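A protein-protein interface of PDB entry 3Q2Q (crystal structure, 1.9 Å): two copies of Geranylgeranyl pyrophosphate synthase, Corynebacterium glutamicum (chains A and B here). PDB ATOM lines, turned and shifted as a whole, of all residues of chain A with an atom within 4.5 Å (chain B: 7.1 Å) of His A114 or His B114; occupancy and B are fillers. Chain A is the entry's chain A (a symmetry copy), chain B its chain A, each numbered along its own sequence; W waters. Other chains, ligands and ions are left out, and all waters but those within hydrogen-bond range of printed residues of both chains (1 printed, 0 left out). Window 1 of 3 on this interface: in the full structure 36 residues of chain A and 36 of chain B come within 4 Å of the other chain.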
ATOM      1  N   ALA A 110     -36.776  13.769 -10.665  1.00  0.00           N
ATOM      2  CA  ALA A 110     -35.755  14.287  -9.750  1.00  0.00           C
ATOM      3  C   ALA A 110     -35.466  15.767 -10.041  1.00  0.00           C
ATOM      4  O   ALA A 110     -35.418  16.604  -9.132  1.00  0.00           O
ATOM      5  CB  ALA A 110     -34.447  13.430  -9.855  1.00  0.00           C
ATOM      6  N   THR A 111     -35.297  16.090 -11.315  1.00  0.00           N
ATOM      7  CA  THR A 111     -34.985  17.462 -11.745  1.00  0.00           C
ATOM      8  C   THR A 111     -36.120  18.438 -11.470  1.00  0.00           C
ATOM      9  O   THR A 111     -35.885  19.577 -11.071  1.00  0.00           O
ATOM     10  CB  THR A 111     -34.589  17.531 -13.245  1.00  0.00           C
ATOM     11  OG1 THR A 111     -35.710  17.187 -14.074  1.00  0.00           O
ATOM     12  CG2 THR A 111     -33.440  16.615 -13.525  1.00  0.00           C
ATOM     13  N   LEU A 112     -37.353  17.992 -11.664  1.00  0.00           N
ATOM     14  CA  LEU A 112     -38.499  18.782 -11.239  1.00  0.00           C
ATOM     15  C   LEU A 112     -38.430  19.116  -9.756  1.00  0.00           C
ATOM     16  O   LEU A 112     -38.721  20.239  -9.358  1.00  0.00           O
ATOM     17  CB  LEU A 112     -39.827  18.057 -11.532  1.00  0.00           C
ATOM     18  CG  LEU A 112     -40.317  18.070 -12.980  1.00  0.00           C
ATOM     19  CD1 LEU A 112     -41.636  17.302 -13.089  1.00  0.00           C
ATOM     20  CD2 LEU A 112     -40.482  19.490 -13.520  1.00  0.00           C
ATOM     21  N   TYR A 113     -38.068  18.144  -8.927  1.00  0.00           N
ATOM     22  CA  TYR A 113     -37.998  18.393  -7.494  1.00  0.00           C
ATOM     23  C   TYR A 113     -36.963  19.462  -7.199  1.00  0.00           C
ATOM     24  O   TYR A 113     -37.208  20.390  -6.414  1.00  0.00           O
ATOM     25  CB  TYR A 113     -37.647  17.118  -6.739  1.00  0.00           C
ATOM     26  CG  TYR A 113     -38.820  16.233  -6.452  1.00  0.00           C
ATOM     27  CD1 TYR A 113     -39.910  16.709  -5.733  1.00  0.00           C
ATOM     28  CD2 TYR A 113     -38.834  14.908  -6.869  1.00  0.00           C
ATOM     29  CE1 TYR A 113     -40.989  15.895  -5.454  1.00  0.00           C
ATOM     30  CE2 TYR A 113     -39.907  14.084  -6.601  1.00  0.00           C
ATOM     31  CZ  TYR A 113     -40.984  14.582  -5.891  1.00  0.00           C
ATOM     32  OH  TYR A 113     -42.061  13.769  -5.614  1.00  0.00           O
ATOM     33  N   HIS A 114     -35.797  19.340  -7.830  1.00  0.00           N
ATOM     34  CA  HIS A 114     -34.753  20.336  -7.629  1.00  0.00           C
ATOM     35  C   HIS A 114     -35.106  21.673  -8.297  1.00  0.00           C
ATOM     36  O   HIS A 114     -34.859  22.736  -7.741  1.00  0.00           O
ATOM     37  CB  HIS A 114     -33.393  19.787  -8.072  1.00  0.00           C
ATOM     38  CG  HIS A 114     -32.862  18.735  -7.149  1.00  0.00           C
ATOM     39  ND1 HIS A 114     -31.610  18.175  -7.295  1.00  0.00           N
ATOM     40  CD2 HIS A 114     -33.400  18.169  -6.041  1.00  0.00           C
ATOM     41  CE1 HIS A 114     -31.411  17.287  -6.336  1.00  0.00           C
ATOM     42  NE2 HIS A 114     -32.480  17.263  -5.561  1.00  0.00           N
ATOM     43  N   ASP A 115     -35.703  21.623  -9.478  1.00  0.00           N
ATOM     44  CA  ASP A 115     -36.158  22.843 -10.128  1.00  0.00           C
ATOM     45  C   ASP A 115     -37.211  23.584  -9.299  1.00  0.00           C
ATOM     46  O   ASP A 115     -37.183  24.809  -9.218  1.00  0.00           O
ATOM     47  CB  ASP A 115     -36.725  22.548 -11.508  1.00  0.00           C
ATOM     48  CG  ASP A 115     -37.270  23.787 -12.174  1.00  0.00           C
ATOM     49  OD1 ASP A 115     -36.476  24.505 -12.813  1.00  0.00           O
ATOM     50  OD2 ASP A 115     -38.488  24.049 -12.041  1.00  0.00           O
ATOM     51  N   ASP A 116     -38.142  22.845  -8.701  1.00  0.00           N
ATOM     52  CA  ASP A 116     -39.208  23.458  -7.904  1.00  0.00           C
ATOM     53  C   ASP A 116     -38.656  24.215  -6.705  1.00  0.00           C
ATOM     54  O   ASP A 116     -39.106  25.320  -6.406  1.00  0.00           O
ATOM     55  CB  ASP A 116     -40.236  22.419  -7.447  1.00  0.00           C
ATOM     56  CG  ASP A 116     -41.105  21.911  -8.590  1.00  0.00           C
ATOM     57  OD1 ASP A 116     -40.979  22.432  -9.722  1.00  0.00           O
ATOM     58  OD2 ASP A 116     -41.914  20.984  -8.358  1.00  0.00           O
ATOM     59  N   VAL A 117     -37.684  23.632  -6.015  1.00  0.00           N
ATOM     60  CA  VAL A 117     -37.088  24.299  -4.858  1.00  0.00           C
ATOM     61  C   VAL A 117     -36.445  25.627  -5.255  1.00  0.00           C
ATOM     62  O   VAL A 117     -36.412  26.577  -4.471  1.00  0.00           O
ATOM     63  CB  VAL A 117     -36.043  23.407  -4.159  1.00  0.00           C
ATOM     64  CG1 VAL A 117     -35.139  24.245  -3.261  1.00  0.00           C
ATOM     65  CG2 VAL A 117     -36.733  22.307  -3.365  1.00  0.00           C
ATOM     66  N   MET A 118     -35.944  25.694  -6.483  1.00  0.00           N
ATOM     67  CA  MET A 118     -35.297  26.906  -6.972  1.00  0.00           C
ATOM     68  C   MET A 118     -36.257  27.941  -7.568  1.00  0.00           C
ATOM     69  O   MET A 118     -35.959  29.135  -7.567  1.00  0.00           O
ATOM     70  CB  MET A 118     -34.192  26.547  -7.955  1.00  0.00           C
ATOM     71  CG  MET A 118     -33.099  25.751  -7.281  1.00  0.00           C
ATOM     72  SD  MET A 118     -31.775  25.317  -8.399  1.00  0.00           S
ATOM     73  CE  MET A 118     -32.724  24.732  -9.808  1.00  0.00           C
ATOM     74  N   ALA A 139     -37.670  18.361  -0.524  1.00  0.00           N
ATOM     75  CA  ALA A 139     -37.680  18.199  -1.969  1.00  0.00           C
ATOM     76  C   ALA A 139     -36.281  17.968  -2.521  1.00  0.00           C
ATOM     77  O   ALA A 139     -36.107  17.260  -3.506  1.00  0.00           O
ATOM     78  CB  ALA A 139     -38.313  19.418  -2.634  1.00  0.00           C
ATOM     79  N   ILE A 140     -35.278  18.583  -1.905  1.00  0.00           N
ATOM     80  CA  ILE A 140     -33.904  18.332  -2.333  1.00  0.00           C
ATOM     81  C   ILE A 140     -33.567  16.849  -2.131  1.00  0.00           C
ATOM     82  O   ILE A 140     -33.013  16.184  -3.022  1.00  0.00           O
ATOM     83  CB  ILE A 140     -32.933  19.173  -1.524  1.00  0.00           C
ATOM     84  CG1 ILE A 140     -33.073  20.643  -1.926  1.00  0.00           C
ATOM     85  CG2 ILE A 140     -31.480  18.717  -1.771  1.00  0.00           C
ATOM     86  CD1 ILE A 140     -32.277  21.591  -0.985  1.00  0.00           C
ATOM     87  N   GLY A 143     -35.419  14.507  -4.499  1.00  0.00           N
ATOM     88  CA  GLY A 143     -34.764  14.447  -5.812  1.00  0.00           C
ATOM     89  C   GLY A 143     -33.545  13.546  -5.739  1.00  0.00           C
ATOM     90  O   GLY A 143     -33.294  12.730  -6.639  1.00  0.00           O
ATOM     91  N   ASP A 144     -32.798  13.668  -4.648  1.00  0.00           N
ATOM     92  CA  ASP A 144     -31.593  12.843  -4.452  1.00  0.00           C
ATOM     93  C   ASP A 144     -31.889  11.335  -4.305  1.00  0.00           C
ATOM     94  O   ASP A 144     -31.170  10.497  -4.861  1.00  0.00           O
ATOM     95  CB  ASP A 144     -30.821  13.334  -3.228  1.00  0.00           C
ATOM     96  CG  ASP A 144     -30.105  14.673  -3.469  1.00  0.00           C
ATOM     97  OD1 ASP A 144     -30.178  15.228  -4.592  1.00  0.00           O
ATOM     98  OD2 ASP A 144     -29.449  15.170  -2.519  1.00  0.00           O
ATOM     99  N   LEU B 109     -18.533  15.539  -1.223  1.00  0.00           N
ATOM    100  CA  LEU B 109     -18.685  16.976  -1.447  1.00  0.00           C
ATOM    101  C   LEU B 109     -20.105  17.332  -1.895  1.00  0.00           C
ATOM    102  O   LEU B 109     -20.655  18.339  -1.478  1.00  0.00           O
ATOM    103  CB  LEU B 109     -17.636  17.508  -2.444  1.00  0.00           C
ATOM    104  CG  LEU B 109     -16.177  17.379  -1.963  1.00  0.00           C
ATOM    105  CD1 LEU B 109     -15.203  17.814  -3.065  1.00  0.00           C
ATOM    106  CD2 LEU B 109     -15.930  18.184  -0.663  1.00  0.00           C
ATOM    107  N   ALA B 110     -20.693  16.503  -2.750  1.00  0.00           N
ATOM    108  CA  ALA B 110     -22.055  16.745  -3.235  1.00  0.00           C
ATOM    109  C   ALA B 110     -23.043  16.820  -2.061  1.00  0.00           C
ATOM    110  O   ALA B 110     -23.875  17.730  -1.978  1.00  0.00           O
ATOM    111  CB  ALA B 110     -22.476  15.627  -4.250  1.00  0.00           C
ATOM    112  N   THR B 111     -22.931  15.872  -1.142  1.00  0.00           N
ATOM    113  CA  THR B 111     -23.825  15.797   0.024  1.00  0.00           C
ATOM    114  C   THR B 111     -23.659  16.976   0.972  1.00  0.00           C
ATOM    115  O   THR B 111     -24.637  17.491   1.511  1.00  0.00           O
ATOM    116  CB  THR B 111     -23.655  14.469   0.809  1.00  0.00           C
ATOM    117  OG1 THR B 111     -22.352  14.404   1.406  1.00  0.00           O
ATOM    118  CG2 THR B 111     -23.867  13.296  -0.096  1.00  0.00           C
ATOM    119  N   LEU B 112     -22.425  17.419   1.164  1.00  0.00           N
ATOM    120  CA  LEU B 112     -22.190  18.659   1.890  1.00  0.00           C
ATOM    121  C   LEU B 112     -22.934  19.827   1.260  1.00  0.00           C
ATOM    122  O   LEU B 112     -23.515  20.646   1.963  1.00  0.00           O
ATOM    123  CB  LEU B 112     -20.688  18.996   1.963  1.00  0.00           C
ATOM    124  CG  LEU B 112     -19.852  18.211   2.974  1.00  0.00           C
ATOM    125  CD1 LEU B 112     -18.391  18.667   2.906  1.00  0.00           C
ATOM    126  CD2 LEU B 112     -20.387  18.350   4.398  1.00  0.00           C
ATOM    127  N   TYR B 113     -22.904  19.927  -0.064  1.00  0.00           N
ATOM    128  CA  TYR B 113     -23.581  21.030  -0.730  1.00  0.00           C
ATOM    129  C   TYR B 113     -25.071  20.974  -0.450  1.00  0.00           C
ATOM    130  O   TYR B 113     -25.701  21.993  -0.131  1.00  0.00           O
ATOM    131  CB  TYR B 113     -23.340  20.988  -2.233  1.00  0.00           C
ATOM    132  CG  TYR B 113     -22.052  21.616  -2.664  1.00  0.00           C
ATOM    133  CD1 TYR B 113     -21.772  22.943  -2.361  1.00  0.00           C
ATOM    134  CD2 TYR B 113     -21.122  20.900  -3.406  1.00  0.00           C
ATOM    135  CE1 TYR B 113     -20.592  23.532  -2.767  1.00  0.00           C
ATOM    136  CE2 TYR B 113     -19.936  21.474  -3.815  1.00  0.00           C
ATOM    137  CZ  TYR B 113     -19.676  22.793  -3.495  1.00  0.00           C
ATOM    138  OH  TYR B 113     -18.498  23.380  -3.900  1.00  0.00           O
ATOM    139  N   HIS B 114     -25.646  19.779  -0.567  1.00  0.00           N
ATOM    140  CA  HIS B 114     -27.068  19.624  -0.290  1.00  0.00           C
ATOM    141  C   HIS B 114     -27.373  19.753   1.210  1.00  0.00           C
ATOM    142  O   HIS B 114     -28.367  20.354   1.597  1.00  0.00           O
ATOM    143  CB  HIS B 114     -27.596  18.320  -0.898  1.00  0.00           C
ATOM    144  CG  HIS B 114     -27.675  18.366  -2.392  1.00  0.00           C
ATOM    145  ND1 HIS B 114     -28.216  17.344  -3.144  1.00  0.00           N
ATOM    146  CD2 HIS B 114     -27.316  19.331  -3.274  1.00  0.00           C
ATOM    147  CE1 HIS B 114     -28.160  17.664  -4.425  1.00  0.00           C
ATOM    148  NE2 HIS B 114     -27.619  18.863  -4.533  1.00  0.00           N
ATOM    149  N   ASP B 115     -26.510  19.210   2.054  1.00  0.00           N
ATOM    150  CA  ASP B 115     -26.676  19.375   3.489  1.00  0.00           C
ATOM    151  C   ASP B 115     -26.617  20.845   3.916  1.00  0.00           C
ATOM    152  O   ASP B 115     -27.387  21.271   4.771  1.00  0.00           O
ATOM    153  CB  ASP B 115     -25.625  18.589   4.257  1.00  0.00           C
ATOM    154  CG  ASP B 115     -25.731  18.802   5.747  1.00  0.00           C
ATOM    155  OD1 ASP B 115     -26.525  18.082   6.385  1.00  0.00           O
ATOM    156  OD2 ASP B 115     -25.035  19.701   6.272  1.00  0.00           O
ATOM    157  N   ASP B 116     -25.696  21.608   3.332  1.00  0.00           N
ATOM    158  CA  ASP B 116     -25.541  23.022   3.683  1.00  0.00           C
ATOM    159  C   ASP B 116     -26.795  23.826   3.371  1.00  0.00           C
ATOM    160  O   ASP B 116     -27.216  24.660   4.171  1.00  0.00           O
ATOM    161  CB  ASP B 116     -24.326  23.644   2.990  1.00  0.00           C
ATOM    162  CG  ASP B 116     -23.005  23.146   3.562  1.00  0.00           C
ATOM    163  OD1 ASP B 116     -23.026  22.391   4.562  1.00  0.00           O
ATOM    164  OD2 ASP B 116     -21.941  23.506   3.009  1.00  0.00           O
ATOM    165  N   VAL B 117     -27.396  23.585   2.213  1.00  0.00           N
ATOM    166  CA  VAL B 117     -28.614  24.303   1.842  1.00  0.00           C
ATOM    167  C   VAL B 117     -29.737  24.043   2.846  1.00  0.00           C
ATOM    168  O   VAL B 117     -30.585  24.906   3.089  1.00  0.00           O
ATOM    169  CB  VAL B 117     -29.091  23.929   0.424  1.00  0.00           C
ATOM    170  CG1 VAL B 117     -30.550  24.327   0.227  1.00  0.00           C
ATOM    171  CG2 VAL B 117     -28.201  24.584  -0.622  1.00  0.00           C
ATOM    172  N   MET B 118     -29.734  22.855   3.437  1.00  0.00           N
ATOM    173  CA  MET B 118     -30.761  22.488   4.405  1.00  0.00           C
ATOM    174  C   MET B 118     -30.467  22.934   5.841  1.00  0.00           C
ATOM    175  O   MET B 118     -31.389  23.132   6.630  1.00  0.00           O
ATOM    176  CB  MET B 118     -31.033  20.992   4.336  1.00  0.00           C
ATOM    177  CG  MET B 118     -31.593  20.601   2.988  1.00  0.00           C
ATOM    178  SD  MET B 118     -31.936  18.853   2.869  1.00  0.00           S
ATOM    179  CE  MET B 118     -30.423  18.179   3.563  1.00  0.00           C
ATOM    180  N   ASP B 119     -29.190  23.092   6.177  1.00  0.00           N
ATOM    181  CA  ASP B 119     -28.821  23.689   7.449  1.00  0.00           C
ATOM    182  C   ASP B 119     -29.391  25.104   7.512  1.00  0.00           C
ATOM    183  O   ASP B 119     -29.507  25.691   8.587  1.00  0.00           O
ATOM    184  CB  ASP B 119     -27.300  23.723   7.619  1.00  0.00           C
ATOM    185  CG  ASP B 119     -26.738  22.395   8.083  1.00  0.00           C
ATOM    186  OD1 ASP B 119     -27.529  21.451   8.294  1.00  0.00           O
ATOM    187  OD2 ASP B 119     -25.502  22.296   8.236  1.00  0.00           O
ATOM    188  N   ASN B 136     -29.107  29.247  -2.750  1.00  0.00           N
ATOM    189  CA  ASN B 136     -29.578  27.892  -2.537  1.00  0.00           C
ATOM    190  C   ASN B 136     -29.704  27.107  -3.843  1.00  0.00           C
ATOM    191  O   ASN B 136     -29.265  25.951  -3.928  1.00  0.00           O
ATOM    192  CB  ASN B 136     -30.886  27.887  -1.734  1.00  0.00           C
ATOM    193  CG  ASN B 136     -30.655  28.097  -0.238  1.00  0.00           C
ATOM    194  OD1 ASN B 136     -29.515  28.212   0.218  1.00  0.00           O
ATOM    195  ND2 ASN B 136     -31.737  28.140   0.528  1.00  0.00           N
ATOM    196  N   SER B 137     -30.287  27.729  -4.863  1.00  0.00           N
ATOM    197  CA  SER B 137     -30.366  27.091  -6.169  1.00  0.00           C
ATOM    198  C   SER B 137     -28.966  26.661  -6.558  1.00  0.00           C
ATOM    199  O   SER B 137     -28.745  25.551  -7.034  1.00  0.00           O
ATOM    200  CB  SER B 137     -30.907  28.061  -7.226  1.00  0.00           C
ATOM    201  OG  SER B 137     -32.260  28.392  -6.973  1.00  0.00           O
ATOM    202  N   ALA B 139     -26.136  26.018  -4.889  1.00  0.00           N
ATOM    203  CA  ALA B 139     -25.550  24.897  -4.171  1.00  0.00           C
ATOM    204  C   ALA B 139     -26.257  23.589  -4.493  1.00  0.00           C
ATOM    205  O   ALA B 139     -25.639  22.531  -4.509  1.00  0.00           O
ATOM    206  CB  ALA B 139     -25.580  25.157  -2.667  1.00  0.00           C
ATOM    207  N   ILE B 140     -27.564  23.648  -4.726  1.00  0.00           N
ATOM    208  CA  ILE B 140     -28.281  22.440  -5.125  1.00  0.00           C
ATOM    209  C   ILE B 140     -27.723  21.929  -6.459  1.00  0.00           C
ATOM    210  O   ILE B 140     -27.440  20.731  -6.624  1.00  0.00           O
ATOM    211  CB  ILE B 140     -29.763  22.734  -5.290  1.00  0.00           C
ATOM    212  CG1 ILE B 140     -30.392  22.977  -3.917  1.00  0.00           C
ATOM    213  CG2 ILE B 140     -30.479  21.550  -5.974  1.00  0.00           C
ATOM    214  CD1 ILE B 140     -31.850  23.504  -4.020  1.00  0.00           C
ATOM    215  N   LEU B 141     -27.559  22.851  -7.406  1.00  0.00           N
ATOM    216  CA  LEU B 141     -27.049  22.513  -8.725  1.00  0.00           C
ATOM    217  C   LEU B 141     -25.576  22.128  -8.700  1.00  0.00           C
ATOM    218  O   LEU B 141     -25.137  21.290  -9.498  1.00  0.00           O
ATOM    219  CB  LEU B 141     -27.277  23.650  -9.713  1.00  0.00           C
ATOM    220  CG  LEU B 141     -28.786  23.923  -9.879  1.00  0.00           C
ATOM    221  CD1 LEU B 141     -28.992  25.147 -10.759  1.00  0.00           C
ATOM    222  CD2 LEU B 141     -29.521  22.690 -10.427  1.00  0.00           C
ATOM    223  N   ALA B 142     -24.805  22.750  -7.814  1.00  0.00           N
ATOM    224  CA  ALA B 142     -23.409  22.342  -7.658  1.00  0.00           C
ATOM    225  C   ALA B 142     -23.343  20.882  -7.179  1.00  0.00           C
ATOM    226  O   ALA B 142     -22.558  20.072  -7.695  1.00  0.00           O
ATOM    227  CB  ALA B 142     -22.685  23.258  -6.694  1.00  0.00           C
ATOM    228  N   GLY B 143     -24.188  20.525  -6.216  1.00  0.00           N
ATOM    229  CA  GLY B 143     -24.195  19.142  -5.722  1.00  0.00           C
ATOM    230  C   GLY B 143     -24.585  18.197  -6.842  1.00  0.00           C
ATOM    231  O   GLY B 143     -23.987  17.123  -7.014  1.00  0.00           O
ATOM    232  N   ASP B 144     -25.571  18.606  -7.631  1.00  0.00           N
ATOM    233  CA  ASP B 144     -26.036  17.785  -8.761  1.00  0.00           C
ATOM    234  C   ASP B 144     -24.979  17.597  -9.871  1.00  0.00           C
ATOM    235  O   ASP B 144     -24.826  16.498 -10.414  1.00  0.00           O
ATOM    236  CB  ASP B 144     -27.303  18.394  -9.361  1.00  0.00           C
ATOM    237  CG  ASP B 144     -28.538  18.212  -8.464  1.00  0.00           C
ATOM    238  OD1 ASP B 144     -28.435  17.591  -7.378  1.00  0.00           O
ATOM    239  OD2 ASP B 144     -29.631  18.687  -8.863  1.00  0.00           O
ATOM    240  N   ILE B 145     -24.240  18.652 -10.221  1.00  0.00           N
ATOM    241  CA  ILE B 145     -23.266  18.498 -11.285  1.00  0.00           C
ATOM    242  C   ILE B 145     -22.162  17.586 -10.767  1.00  0.00           C
ATOM    243  O   ILE B 145     -21.602  16.777 -11.532  1.00  0.00           O
ATOM    244  CB  ILE B 145     -22.678  19.847 -11.823  1.00  0.00           C
ATOM    245  CG1 ILE B 145     -21.952  19.616 -13.151  1.00  0.00           C
ATOM    246  CG2 ILE B 145     -21.679  20.476 -10.826  1.00  0.00           C
ATOM    247  CD1 ILE B 145     -22.869  19.195 -14.315  1.00  0.00           C
ATOM    248  N   LEU B 147     -22.589  15.009  -8.777  1.00  0.00           N
ATOM    249  CA  LEU B 147     -23.097  13.641  -8.948  1.00  0.00           C
ATOM    250  C   LEU B 147     -22.986  13.211 -10.396  1.00  0.00           C
ATOM    251  O   LEU B 147     -22.680  12.055 -10.667  1.00  0.00           O
ATOM    252  CB  LEU B 147     -24.558  13.503  -8.464  1.00  0.00           C
ATOM    253  CG  LEU B 147     -24.714  13.862  -6.969  1.00  0.00           C
ATOM    254  CD1 LEU B 147     -26.168  14.110  -6.580  1.00  0.00           C
ATOM    255  CD2 LEU B 147     -24.095  12.811  -6.034  1.00  0.00           C
ATOM    256  N   PHE B 169     -25.265   5.798  -1.764  1.00  0.00           N
ATOM    257  CA  PHE B 169     -25.867   7.121  -1.862  1.00  0.00           C
ATOM    258  C   PHE B 169     -27.334   7.108  -1.360  1.00  0.00           C
ATOM    259  O   PHE B 169     -27.772   8.028  -0.675  1.00  0.00           O
ATOM    260  CB  PHE B 169     -25.747   7.645  -3.310  1.00  0.00           C
ATOM    261  CG  PHE B 169     -26.282   9.038  -3.511  1.00  0.00           C
ATOM    262  CD1 PHE B 169     -25.759  10.112  -2.817  1.00  0.00           C
ATOM    263  CD2 PHE B 169     -27.300   9.272  -4.420  1.00  0.00           C
ATOM    264  CE1 PHE B 169     -26.257  11.404  -3.018  1.00  0.00           C
ATOM    265  CE2 PHE B 169     -27.814  10.560  -4.620  1.00  0.00           C
ATOM    266  CZ  PHE B 169     -27.279  11.626  -3.915  1.00  0.00           C
ATOM    267  N   VAL B 173     -28.601   9.478   1.680  1.00  0.00           N
ATOM    268  CA  VAL B 173     -29.769  10.333   1.554  1.00  0.00           C
ATOM    269  C   VAL B 173     -30.842   9.968   2.588  1.00  0.00           C
ATOM    270  O   VAL B 173     -31.484  10.847   3.148  1.00  0.00           O
ATOM    271  CB  VAL B 173     -30.393  10.283   0.130  1.00  0.00           C
ATOM    272  CG1 VAL B 173     -31.723  11.065   0.100  1.00  0.00           C
ATOM    273  CG2 VAL B 173     -29.404  10.837  -0.909  1.00  0.00           C
ATOM    274  N   GLN B 176     -29.827  11.660   5.889  1.00  0.00           N
ATOM    275  CA  GLN B 176     -30.191  13.075   5.883  1.00  0.00           C
ATOM    276  C   GLN B 176     -31.710  13.244   6.072  1.00  0.00           C
ATOM    277  O   GLN B 176     -32.141  14.103   6.822  1.00  0.00           O
ATOM    278  CB  GLN B 176     -29.733  13.762   4.587  1.00  0.00           C
ATOM    279  CG  GLN B 176     -28.206  13.853   4.414  1.00  0.00           C
ATOM    280  CD  GLN B 176     -27.803  14.210   2.984  1.00  0.00           C
ATOM    281  OE1 GLN B 176     -28.030  13.437   2.050  1.00  0.00           O
ATOM    282  NE2 GLN B 176     -27.200  15.378   2.807  1.00  0.00           N
HETATM  283  O   HOH W   1     -27.472  14.692  -0.529  1.00  0.00           O
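Among the printed residues, pairs that only touch across the chains: His A114 with His B114 (3.8 Å), His A114 with Ile B140 (3.8 Å), Val A117 with Ile B140 (3.5 Å), Met A118 with Leu B141 (3.6 Å), Ile A140 with His B114 (3.8 Å), Ile A140 with Val B117 (3.5 Å), Ile A140 with Ile B140 (3.6 Å), Asp A144 with Phe B169 (3.4 Å) and Asp A144 with Val B173 (3.7 Å).
Hydrophobic or aromatic side chains of chain B that line the printed part of chain A: His B114, Val B117, Ile B140, Leu B141, Phe B169 and Val B173. Among the printed residues, 12 pairs touch across the chains.
His A114 touches its own counterpart, His B114. His A114 touches Ile B140, and with the chains exchanged Ile A140 touches His B114. Val A117 touches Ile B140, and with the chains exchanged Ile A140 touches Val B117. Ile B140 touches its own counterpart, Ile A140. Of the 12 pairs that touch across the chains among the printed residues, 8 have their exchanged pair printed and touching as well.
Of chain B, only His B114, Ile B140 and Asp B144 come within 4 Å of His A114. His B114 touches three residues of chain A. Printed residues of chain A within 4 Å of Ile B140: His A114 (3.8 Å), Val A117 (3.5 Å) and Ile A140 (3.6 Å). Of the printed residues of chain B, Val A117 touches Ile B140. Printed residues of chain B within 4 Å of Asp A144: His B114, Phe B169 and Val B173. Of the printed residues of chain A, Phe B169 touches Asp A144 (3.4 Å). The nearest printed residue of chain A that does not touch His B114 is Gly A143 (6.9 Å). The nearest printed residue of chain A that does not touch Leu B141 is His A114 (5.4 Å).
Water W1 lies within hydrogen-bond range of the side-chain carboxylate (OD2) of Asp A144 (2.8 Å) and the side-chain amide oxygen (OE1) of Gln B176 (2.9 Å).
The side-chain sulfur (SD) of Met A118 sits close to the side-chain hydroxyl (OG) of Ser B137 (3.4 Å). A ring nitrogen (ND1) of His B114 is in hydrogen-bond range of the side-chain carboxylate of Asp A144 (2.6 Å). The side-chain carboxylate (OD2) of Asp B144 is in hydrogen-bond range of a ring nitrogen (ND1) of His A114 (2.6 Å).
NE2 of His A114 lies close to OD1 of Asp A144 (3.2 Å). A ring nitrogen (NE2) of His B114 lies close to the side-chain carboxylate (OD1) of Asp B144. The backbone carbonyl oxygen (O) of Ile A140 is in hydrogen-bond range of a ring nitrogen (NE2) of His A114. The backbone carbonyl oxygen of Ile B140 sits at hydrogen-bond distance from a ring nitrogen (NE2) of His B114 (2.8 Å).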
